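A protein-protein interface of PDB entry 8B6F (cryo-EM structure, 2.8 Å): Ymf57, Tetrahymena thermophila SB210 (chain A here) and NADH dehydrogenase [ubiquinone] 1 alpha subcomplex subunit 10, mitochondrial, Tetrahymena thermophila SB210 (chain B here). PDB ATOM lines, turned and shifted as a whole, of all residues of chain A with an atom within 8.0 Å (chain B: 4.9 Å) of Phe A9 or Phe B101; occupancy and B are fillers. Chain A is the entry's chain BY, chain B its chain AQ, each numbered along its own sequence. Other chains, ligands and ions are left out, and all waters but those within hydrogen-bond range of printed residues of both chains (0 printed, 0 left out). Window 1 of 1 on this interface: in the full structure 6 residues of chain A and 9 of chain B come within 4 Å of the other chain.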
ATOM      1  N   LYS A   5     -38.506  10.270 -21.437  1.00  0.00           N
ATOM      2  CA  LYS A   5     -37.059  10.195 -21.315  1.00  0.00           C
ATOM      3  C   LYS A   5     -36.366  11.509 -21.635  1.00  0.00           C
ATOM      4  O   LYS A   5     -35.178  11.655 -21.330  1.00  0.00           O
ATOM      5  CB  LYS A   5     -36.517   9.096 -22.237  1.00  0.00           C
ATOM      6  CG  LYS A   5     -35.105   8.634 -21.910  1.00  0.00           C
ATOM      7  CD  LYS A   5     -35.055   7.777 -20.653  1.00  0.00           C
ATOM      8  CE  LYS A   5     -35.601   6.378 -20.890  1.00  0.00           C
ATOM      9  NZ  LYS A   5     -34.792   5.617 -21.885  1.00  0.00           N
ATOM     10  N   LEU A   6     -37.072  12.470 -22.233  1.00  0.00           N
ATOM     11  CA  LEU A   6     -36.441  13.727 -22.612  1.00  0.00           C
ATOM     12  C   LEU A   6     -36.179  14.631 -21.414  1.00  0.00           C
ATOM     13  O   LEU A   6     -35.297  15.494 -21.489  1.00  0.00           O
ATOM     14  CB  LEU A   6     -37.309  14.463 -23.635  1.00  0.00           C
ATOM     15  CG  LEU A   6     -37.290  13.927 -25.070  1.00  0.00           C
ATOM     16  CD1 LEU A   6     -37.811  12.503 -25.140  1.00  0.00           C
ATOM     17  CD2 LEU A   6     -38.095  14.826 -25.992  1.00  0.00           C
ATOM     18  N   ILE A   7     -36.924  14.466 -20.318  1.00  0.00           N
ATOM     19  CA  ILE A   7     -36.692  15.281 -19.127  1.00  0.00           C
ATOM     20  C   ILE A   7     -35.487  14.824 -18.326  1.00  0.00           C
ATOM     21  O   ILE A   7     -35.056  15.539 -17.413  1.00  0.00           O
ATOM     22  CB  ILE A   7     -37.920  15.288 -18.198  1.00  0.00           C
ATOM     23  CG1 ILE A   7     -38.265  13.861 -17.755  1.00  0.00           C
ATOM     24  CG2 ILE A   7     -39.100  15.938 -18.902  1.00  0.00           C
ATOM     25  CD1 ILE A   7     -39.395  13.780 -16.758  1.00  0.00           C
ATOM     26  N   LYS A   8     -34.932  13.656 -18.633  1.00  0.00           N
ATOM     27  CA  LYS A   8     -33.817  13.135 -17.860  1.00  0.00           C
ATOM     28  C   LYS A   8     -32.540  13.905 -18.169  1.00  0.00           C
ATOM     29  O   LYS A   8     -32.382  14.489 -19.245  1.00  0.00           O
ATOM     30  CB  LYS A   8     -33.617  11.648 -18.144  1.00  0.00           C
ATOM     31  CG  LYS A   8     -34.824  10.802 -17.784  1.00  0.00           C
ATOM     32  CD  LYS A   8     -34.479   9.323 -17.718  1.00  0.00           C
ATOM     33  CE  LYS A   8     -33.698   8.978 -16.460  1.00  0.00           C
ATOM     34  NZ  LYS A   8     -34.455   9.290 -15.215  1.00  0.00           N
ATOM     35  N   PHE A   9     -31.617  13.898 -17.206  1.00  0.00           N
ATOM     36  CA  PHE A   9     -30.414  14.710 -17.333  1.00  0.00           C
ATOM     37  C   PHE A   9     -29.531  14.249 -18.486  1.00  0.00           C
ATOM     38  O   PHE A   9     -28.755  15.045 -19.022  1.00  0.00           O
ATOM     39  CB  PHE A   9     -29.622  14.696 -16.029  1.00  0.00           C
ATOM     40  CG  PHE A   9     -28.451  15.631 -16.032  1.00  0.00           C
ATOM     41  CD1 PHE A   9     -28.637  16.993 -15.871  1.00  0.00           C
ATOM     42  CD2 PHE A   9     -27.165  15.152 -16.208  1.00  0.00           C
ATOM     43  CE1 PHE A   9     -27.564  17.858 -15.880  1.00  0.00           C
ATOM     44  CE2 PHE A   9     -26.088  16.011 -16.219  1.00  0.00           C
ATOM     45  CZ  PHE A   9     -26.288  17.366 -16.053  1.00  0.00           C
ATOM     46  N   LYS A  10     -29.624  12.978 -18.881  1.00  0.00           N
ATOM     47  CA  LYS A  10     -28.835  12.512 -20.016  1.00  0.00           C
ATOM     48  C   LYS A  10     -29.203  13.284 -21.276  1.00  0.00           C
ATOM     49  O   LYS A  10     -28.332  13.838 -21.955  1.00  0.00           O
ATOM     50  CB  LYS A  10     -29.038  11.012 -20.224  1.00  0.00           C
ATOM     51  CG  LYS A  10     -28.165  10.434 -21.327  1.00  0.00           C
ATOM     52  CD  LYS A  10     -28.296   8.924 -21.426  1.00  0.00           C
ATOM     53  CE  LYS A  10     -29.687   8.517 -21.881  1.00  0.00           C
ATOM     54  NZ  LYS A  10     -29.796   7.046 -22.084  1.00  0.00           N
ATOM     55  N   PHE A  11     -30.492  13.322 -21.613  1.00  0.00           N
ATOM     56  CA  PHE A  11     -30.922  14.101 -22.769  1.00  0.00           C
ATOM     57  C   PHE A  11     -30.691  15.590 -22.545  1.00  0.00           C
ATOM     58  O   PHE A  11     -30.325  16.312 -23.477  1.00  0.00           O
ATOM     59  CB  PHE A  11     -32.392  13.828 -23.073  1.00  0.00           C
ATOM     60  CG  PHE A  11     -32.911  14.585 -24.260  1.00  0.00           C
ATOM     61  CD1 PHE A  11     -32.734  14.095 -25.542  1.00  0.00           C
ATOM     62  CD2 PHE A  11     -33.582  15.784 -24.092  1.00  0.00           C
ATOM     63  CE1 PHE A  11     -33.212  14.790 -26.635  1.00  0.00           C
ATOM     64  CE2 PHE A  11     -34.061  16.483 -25.181  1.00  0.00           C
ATOM     65  CZ  PHE A  11     -33.877  15.984 -26.453  1.00  0.00           C
ATOM     66  N   PHE A  12     -30.898  16.067 -21.317  1.00  0.00           N
ATOM     67  CA  PHE A  12     -30.699  17.482 -21.032  1.00  0.00           C
ATOM     68  C   PHE A  12     -29.276  17.913 -21.361  1.00  0.00           C
ATOM     69  O   PHE A  12     -29.060  18.912 -22.056  1.00  0.00           O
ATOM     70  CB  PHE A  12     -31.022  17.779 -19.568  1.00  0.00           C
ATOM     71  CG  PHE A  12     -31.048  19.243 -19.244  1.00  0.00           C
ATOM     72  CD1 PHE A  12     -32.219  19.970 -19.374  1.00  0.00           C
ATOM     73  CD2 PHE A  12     -29.904  19.895 -18.822  1.00  0.00           C
ATOM     74  CE1 PHE A  12     -32.251  21.318 -19.085  1.00  0.00           C
ATOM     75  CE2 PHE A  12     -29.929  21.246 -18.530  1.00  0.00           C
ATOM     76  CZ  PHE A  12     -31.105  21.957 -18.662  1.00  0.00           C
ATOM     77  N   ARG A  13     -28.286  17.161 -20.877  1.00  0.00           N
ATOM     78  CA  ARG A  13     -26.897  17.521 -21.141  1.00  0.00           C
ATOM     79  C   ARG A  13     -26.522  17.287 -22.597  1.00  0.00           C
ATOM     80  O   ARG A  13     -25.695  18.026 -23.143  1.00  0.00           O
ATOM     81  CB  ARG A  13     -25.961  16.749 -20.212  1.00  0.00           C
ATOM     82  CG  ARG A  13     -25.847  15.268 -20.511  1.00  0.00           C
ATOM     83  CD  ARG A  13     -24.932  14.587 -19.510  1.00  0.00           C
ATOM     84  NE  ARG A  13     -24.765  13.171 -19.803  1.00  0.00           N
ATOM     85  CZ  ARG A  13     -24.111  12.315 -19.030  1.00  0.00           C
ATOM     86  NH1 ARG A  13     -23.551  12.698 -17.896  1.00  0.00           N
ATOM     87  NH2 ARG A  13     -24.022  11.042 -19.402  1.00  0.00           N
ATOM     88  N   PHE A  14     -27.096  16.271 -23.241  1.00  0.00           N
ATOM     89  CA  PHE A  14     -26.857  16.095 -24.668  1.00  0.00           C
ATOM     90  C   PHE A  14     -27.245  17.346 -25.444  1.00  0.00           C
ATOM     91  O   PHE A  14     -26.490  17.820 -26.300  1.00  0.00           O
ATOM     92  CB  PHE A  14     -27.638  14.890 -25.193  1.00  0.00           C
ATOM     93  CG  PHE A  14     -28.015  15.008 -26.640  1.00  0.00           C
ATOM     94  CD1 PHE A  14     -27.101  14.710 -27.633  1.00  0.00           C
ATOM     95  CD2 PHE A  14     -29.279  15.436 -27.007  1.00  0.00           C
ATOM     96  CE1 PHE A  14     -27.443  14.826 -28.964  1.00  0.00           C
ATOM     97  CE2 PHE A  14     -29.627  15.554 -28.336  1.00  0.00           C
ATOM     98  CZ  PHE A  14     -28.708  15.250 -29.315  1.00  0.00           C
ATOM     99  N   VAL A  15     -28.431  17.889 -25.169  1.00  0.00           N
ATOM    100  CA  VAL A  15     -28.876  19.076 -25.889  1.00  0.00           C
ATOM    101  C   VAL A  15     -28.062  20.291 -25.465  1.00  0.00           C
ATOM    102  O   VAL A  15     -27.728  21.151 -26.288  1.00  0.00           O
ATOM    103  CB  VAL A  15     -30.385  19.302 -25.688  1.00  0.00           C
ATOM    104  CG1 VAL A  15     -30.840  20.516 -26.470  1.00  0.00           C
ATOM    105  CG2 VAL A  15     -31.174  18.079 -26.111  1.00  0.00           C
ATOM    106  N   GLN A  16     -27.735  20.388 -24.173  1.00  0.00           N
ATOM    107  CA  GLN A  16     -26.968  21.532 -23.694  1.00  0.00           C
ATOM    108  C   GLN A  16     -25.582  21.579 -24.320  1.00  0.00           C
ATOM    109  O   GLN A  16     -25.031  22.665 -24.529  1.00  0.00           O
ATOM    110  CB  GLN A  16     -26.856  21.490 -22.171  1.00  0.00           C
ATOM    111  CG  GLN A  16     -26.034  22.630 -21.584  1.00  0.00           C
ATOM    112  CD  GLN A  16     -26.064  22.664 -20.067  1.00  0.00           C
ATOM    113  OE1 GLN A  16     -25.998  23.734 -19.463  1.00  0.00           O
ATOM    114  NE2 GLN A  16     -26.156  21.494 -19.441  1.00  0.00           N
ATOM    115  N   SER A  17     -25.000  20.420 -24.626  1.00  0.00           N
ATOM    116  CA  SER A  17     -23.669  20.349 -25.213  1.00  0.00           C
ATOM    117  C   SER A  17     -23.674  20.597 -26.712  1.00  0.00           C
ATOM    118  O   SER A  17     -22.687  20.278 -27.383  1.00  0.00           O
ATOM    119  CB  SER A  17     -23.037  18.987 -24.919  1.00  0.00           C
ATOM    120  OG  SER A  17     -22.960  18.754 -23.525  1.00  0.00           O
ATOM    121  N   TYR A  20     -23.151  17.448 -29.103  1.00  0.00           N
ATOM    122  CA  TYR A  20     -21.817  16.861 -29.169  1.00  0.00           C
ATOM    123  C   TYR A  20     -21.103  17.168 -30.480  1.00  0.00           C
ATOM    124  O   TYR A  20     -20.073  16.552 -30.776  1.00  0.00           O
ATOM    125  CB  TYR A  20     -21.869  15.344 -28.956  1.00  0.00           C
ATOM    126  CG  TYR A  20     -22.556  14.924 -27.679  1.00  0.00           C
ATOM    127  CD1 TYR A  20     -22.378  15.639 -26.502  1.00  0.00           C
ATOM    128  CD2 TYR A  20     -23.389  13.815 -27.653  1.00  0.00           C
ATOM    129  CE1 TYR A  20     -23.004  15.258 -25.333  1.00  0.00           C
ATOM    130  CE2 TYR A  20     -24.020  13.426 -26.490  1.00  0.00           C
ATOM    131  CZ  TYR A  20     -23.824  14.150 -25.334  1.00  0.00           C
ATOM    132  OH  TYR A  20     -24.452  13.764 -24.175  1.00  0.00           O
ATOM    133  N   PHE B   7     -11.009  18.846 -17.986  1.00  0.00           N
ATOM    134  CA  PHE B   7     -11.261  18.971 -19.413  1.00  0.00           C
ATOM    135  C   PHE B   7     -10.028  19.402 -20.189  1.00  0.00           C
ATOM    136  O   PHE B   7     -10.124  19.670 -21.390  1.00  0.00           O
ATOM    137  CB  PHE B   7     -12.404  19.960 -19.643  1.00  0.00           C
ATOM    138  CG  PHE B   7     -13.604  19.697 -18.780  1.00  0.00           C
ATOM    139  CD1 PHE B   7     -14.005  18.400 -18.506  1.00  0.00           C
ATOM    140  CD2 PHE B   7     -14.317  20.745 -18.226  1.00  0.00           C
ATOM    141  CE1 PHE B   7     -15.099  18.153 -17.709  1.00  0.00           C
ATOM    142  CE2 PHE B   7     -15.414  20.504 -17.426  1.00  0.00           C
ATOM    143  CZ  PHE B   7     -15.806  19.206 -17.169  1.00  0.00           C
ATOM    144  N   TRP B  13     -11.648   9.135 -20.058  1.00  0.00           N
ATOM    145  CA  TRP B  13     -12.858   9.145 -19.242  1.00  0.00           C
ATOM    146  C   TRP B  13     -12.614   8.504 -17.883  1.00  0.00           C
ATOM    147  O   TRP B  13     -13.104   8.997 -16.861  1.00  0.00           O
ATOM    148  CB  TRP B  13     -14.001   8.431 -19.958  1.00  0.00           C
ATOM    149  CG  TRP B  13     -15.120   8.120 -19.020  1.00  0.00           C
ATOM    150  CD1 TRP B  13     -15.664   6.896 -18.768  1.00  0.00           C
ATOM    151  CD2 TRP B  13     -15.813   9.049 -18.179  1.00  0.00           C
ATOM    152  NE1 TRP B  13     -16.660   7.008 -17.830  1.00  0.00           N
ATOM    153  CE2 TRP B  13     -16.772   8.320 -17.454  1.00  0.00           C
ATOM    154  CE3 TRP B  13     -15.719  10.429 -17.976  1.00  0.00           C
ATOM    155  CZ2 TRP B  13     -17.632   8.923 -16.541  1.00  0.00           C
ATOM    156  CZ3 TRP B  13     -16.574  11.027 -17.068  1.00  0.00           C
ATOM    157  CH2 TRP B  13     -17.520  10.275 -16.363  1.00  0.00           C
ATOM    158  N   VAL B  16     -10.780  10.992 -15.731  1.00  0.00           N
ATOM    159  CA  VAL B  16     -11.662  12.078 -15.314  1.00  0.00           C
ATOM    160  C   VAL B  16     -12.617  11.598 -14.233  1.00  0.00           C
ATOM    161  O   VAL B  16     -12.883  12.310 -13.257  1.00  0.00           O
ATOM    162  CB  VAL B  16     -12.423  12.657 -16.522  1.00  0.00           C
ATOM    163  CG1 VAL B  16     -13.482  13.658 -16.060  1.00  0.00           C
ATOM    164  CG2 VAL B  16     -11.460  13.315 -17.489  1.00  0.00           C
ATOM    165  N   LEU B  20     -12.930  13.096 -10.474  1.00  0.00           N
ATOM    166  CA  LEU B  20     -14.172  13.613  -9.912  1.00  0.00           C
ATOM    167  C   LEU B  20     -14.520  12.914  -8.605  1.00  0.00           C
ATOM    168  O   LEU B  20     -14.843  13.566  -7.605  1.00  0.00           O
ATOM    169  CB  LEU B  20     -15.305  13.448 -10.924  1.00  0.00           C
ATOM    170  CG  LEU B  20     -15.189  14.280 -12.203  1.00  0.00           C
ATOM    171  CD1 LEU B  20     -16.279  13.904 -13.188  1.00  0.00           C
ATOM    172  CD2 LEU B  20     -15.244  15.762 -11.892  1.00  0.00           C
ATOM    173  N   HIS B  50     -26.582  19.765  -8.125  1.00  0.00           N
ATOM    174  CA  HIS B  50     -27.723  19.443  -8.974  1.00  0.00           C
ATOM    175  C   HIS B  50     -29.073  19.651  -8.303  1.00  0.00           C
ATOM    176  O   HIS B  50     -30.065  19.856  -9.009  1.00  0.00           O
ATOM    177  CB  HIS B  50     -27.631  17.992  -9.453  1.00  0.00           C
ATOM    178  CG  HIS B  50     -26.741  17.807 -10.639  1.00  0.00           C
ATOM    179  ND1 HIS B  50     -25.374  17.977 -10.576  1.00  0.00           N
ATOM    180  CD2 HIS B  50     -27.020  17.480 -11.921  1.00  0.00           C
ATOM    181  CE1 HIS B  50     -24.850  17.757 -11.767  1.00  0.00           C
ATOM    182  NE2 HIS B  50     -25.828  17.452 -12.602  1.00  0.00           N
ATOM    183  N   LEU B  96     -23.320   6.966 -10.180  1.00  0.00           N
ATOM    184  CA  LEU B  96     -24.086   8.172  -9.892  1.00  0.00           C
ATOM    185  C   LEU B  96     -23.305   9.416 -10.289  1.00  0.00           C
ATOM    186  O   LEU B  96     -23.867  10.354 -10.867  1.00  0.00           O
ATOM    187  CB  LEU B  96     -24.460   8.207  -8.408  1.00  0.00           C
ATOM    188  CG  LEU B  96     -25.409   9.307  -7.913  1.00  0.00           C
ATOM    189  CD1 LEU B  96     -26.055   8.880  -6.607  1.00  0.00           C
ATOM    190  CD2 LEU B  96     -24.710  10.644  -7.717  1.00  0.00           C
ATOM    191  N   GLN B  97     -22.008   9.446  -9.983  1.00  0.00           N
ATOM    192  CA  GLN B  97     -21.187  10.582 -10.384  1.00  0.00           C
ATOM    193  C   GLN B  97     -21.160  10.724 -11.901  1.00  0.00           C
ATOM    194  O   GLN B  97     -21.259  11.837 -12.431  1.00  0.00           O
ATOM    195  CB  GLN B  97     -19.770  10.416  -9.834  1.00  0.00           C
ATOM    196  CG  GLN B  97     -18.880  11.630 -10.018  1.00  0.00           C
ATOM    197  CD  GLN B  97     -19.276  12.777  -9.116  1.00  0.00           C
ATOM    198  OE1 GLN B  97     -20.080  12.613  -8.201  1.00  0.00           O
ATOM    199  NE2 GLN B  97     -18.710  13.950  -9.370  1.00  0.00           N
ATOM    200  N   GLU B  98     -21.018   9.607 -12.616  1.00  0.00           N
ATOM    201  CA  GLU B  98     -21.038   9.659 -14.073  1.00  0.00           C
ATOM    202  C   GLU B  98     -22.383  10.155 -14.584  1.00  0.00           C
ATOM    203  O   GLU B  98     -22.444  10.964 -15.515  1.00  0.00           O
ATOM    204  CB  GLU B  98     -20.715   8.280 -14.651  1.00  0.00           C
ATOM    205  CG  GLU B  98     -20.785   8.207 -16.173  1.00  0.00           C
ATOM    206  CD  GLU B  98     -22.186   7.961 -16.701  1.00  0.00           C
ATOM    207  OE1 GLU B  98     -23.084   7.643 -15.894  1.00  0.00           O
ATOM    208  OE2 GLU B  98     -22.390   8.088 -17.926  1.00  0.00           O
ATOM    209  N   GLU B  99     -23.477   9.673 -13.988  1.00  0.00           N
ATOM    210  CA  GLU B  99     -24.806  10.099 -14.413  1.00  0.00           C
ATOM    211  C   GLU B  99     -24.996  11.596 -14.221  1.00  0.00           C
ATOM    212  O   GLU B  99     -25.552  12.275 -15.090  1.00  0.00           O
ATOM    213  CB  GLU B  99     -25.870   9.322 -13.636  1.00  0.00           C
ATOM    214  CG  GLU B  99     -27.298   9.786 -13.885  1.00  0.00           C
ATOM    215  CD  GLU B  99     -28.302   9.034 -13.036  1.00  0.00           C
ATOM    216  OE1 GLU B  99     -27.880   8.140 -12.274  1.00  0.00           O
ATOM    217  OE2 GLU B  99     -29.509   9.338 -13.128  1.00  0.00           O
ATOM    218  N   LEU B 100     -24.546  12.128 -13.090  1.00  0.00           N
ATOM    219  CA  LEU B 100     -24.676  13.550 -12.809  1.00  0.00           C
ATOM    220  C   LEU B 100     -23.579  14.383 -13.456  1.00  0.00           C
ATOM    221  O   LEU B 100     -23.616  15.611 -13.343  1.00  0.00           O
ATOM    222  CB  LEU B 100     -24.683  13.789 -11.296  1.00  0.00           C
ATOM    223  CG  LEU B 100     -25.882  13.230 -10.521  1.00  0.00           C
ATOM    224  CD1 LEU B 100     -25.765  13.556  -9.044  1.00  0.00           C
ATOM    225  CD2 LEU B 100     -27.197  13.759 -11.066  1.00  0.00           C
ATOM    226  N   PHE B 101     -22.612  13.760 -14.125  1.00  0.00           N
ATOM    227  CA  PHE B 101     -21.570  14.523 -14.797  1.00  0.00           C
ATOM    228  C   PHE B 101     -22.193  15.522 -15.761  1.00  0.00           C
ATOM    229  O   PHE B 101     -23.028  15.163 -16.594  1.00  0.00           O
ATOM    230  CB  PHE B 101     -20.621  13.593 -15.550  1.00  0.00           C
ATOM    231  CG  PHE B 101     -19.591  14.317 -16.369  1.00  0.00           C
ATOM    232  CD1 PHE B 101     -18.426  14.782 -15.786  1.00  0.00           C
ATOM    233  CD2 PHE B 101     -19.793  14.538 -17.720  1.00  0.00           C
ATOM    234  CE1 PHE B 101     -17.481  15.451 -16.535  1.00  0.00           C
ATOM    235  CE2 PHE B 101     -18.851  15.207 -18.473  1.00  0.00           C
ATOM    236  CZ  PHE B 101     -17.694  15.663 -17.880  1.00  0.00           C
ATOM    237  N   ASP B 102     -21.773  16.775 -15.646  1.00  0.00           N
ATOM    238  CA  ASP B 102     -22.319  17.868 -16.446  1.00  0.00           C
ATOM    239  C   ASP B 102     -21.186  18.576 -17.172  1.00  0.00           C
ATOM    240  O   ASP B 102     -20.361  19.244 -16.516  1.00  0.00           O
ATOM    241  CB  ASP B 102     -23.080  18.848 -15.559  1.00  0.00           C
ATOM    242  CG  ASP B 102     -23.743  19.956 -16.349  1.00  0.00           C
ATOM    243  OD1 ASP B 102     -23.699  19.910 -17.596  1.00  0.00           O
ATOM    244  OD2 ASP B 102     -24.308  20.876 -15.722  1.00  0.00           O
ATOM    245  N   PRO B 103     -21.092  18.469 -18.495  1.00  0.00           N
ATOM    246  CA  PRO B 103     -20.138  19.312 -19.217  1.00  0.00           C
ATOM    247  C   PRO B 103     -20.436  20.780 -18.958  1.00  0.00           C
ATOM    248  O   PRO B 103     -21.594  21.187 -18.843  1.00  0.00           O
ATOM    249  CB  PRO B 103     -20.362  18.932 -20.685  1.00  0.00           C
ATOM    250  CG  PRO B 103     -20.933  17.565 -20.639  1.00  0.00           C
ATOM    251  CD  PRO B 103     -21.763  17.510 -19.389  1.00  0.00           C
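O of Glu B99 is in hydrogen-bond range of NH1 of Arg A13, at 3.5 Å.
The side-chain carboxylate (OD1) of Asp B102 is in hydrogen-bond range of the side-chain amide nitrogen (NE2) of Gln A16 (3.5 Å).
The backbone carbonyl oxygen (O) of Phe B101 lies within hydrogen-bond range of the guanidinium group (NH1) of Arg A13, at 2.8 Å.
OE2 of Glu B98 lies within salt-bridge range of NH2 of Arg A13, at 3.7 Å.
A ring nitrogen (NE2) of His B50 lies close to the backbone carbonyl oxygen (O) of Leu B100 (3.0 Å).
OG of Ser A17 lies within hydrogen-bond range of O of Arg A13.
Among the printed residues, merely in contact across the chains: Phe A9 with His B50 (3.5 Å), Phe A9 with Glu B99 (3.5 Å), Phe A9 with Leu B100 (3.8 Å), Phe A9 with Phe B101 (3.2 Å), Phe A9 with Asp B102 (3.6 Å) and Ser A17 with Pro B103 (3.7 Å).
Of the printed residues of chain B, Phe A9 touches His B50 (3.5 Å), Glu B99 (3.5 Å), Leu B100 (3.8 Å), Phe B101 (3.2 Å) and Asp B102 (3.6 Å).
Phe B101 touches just these residues of chain A: Phe A9 (3.2 Å) and Arg A13 (2.8 Å).
Printed residues of chain A within 4 Å of Leu B100: Phe A9.
Of the printed residues of chain A, Glu B98 touches Arg A13.
Of the printed residues of chain B, Arg A13 touches Glu B98 (3.1 Å), Glu B99 (3.5 Å) and Phe B101 (2.8 Å).
The nearest residue of chain A that does not touch Phe B101 is Lys A10 (7.2 Å).
Among the printed residues, 10 pairs touch across the chains.
Among the printed residues, Asp or Glu carboxylates within 4 Å of a Lys or Arg side-chain nitrogen of the other chain: Arg A13 with Glu B98.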
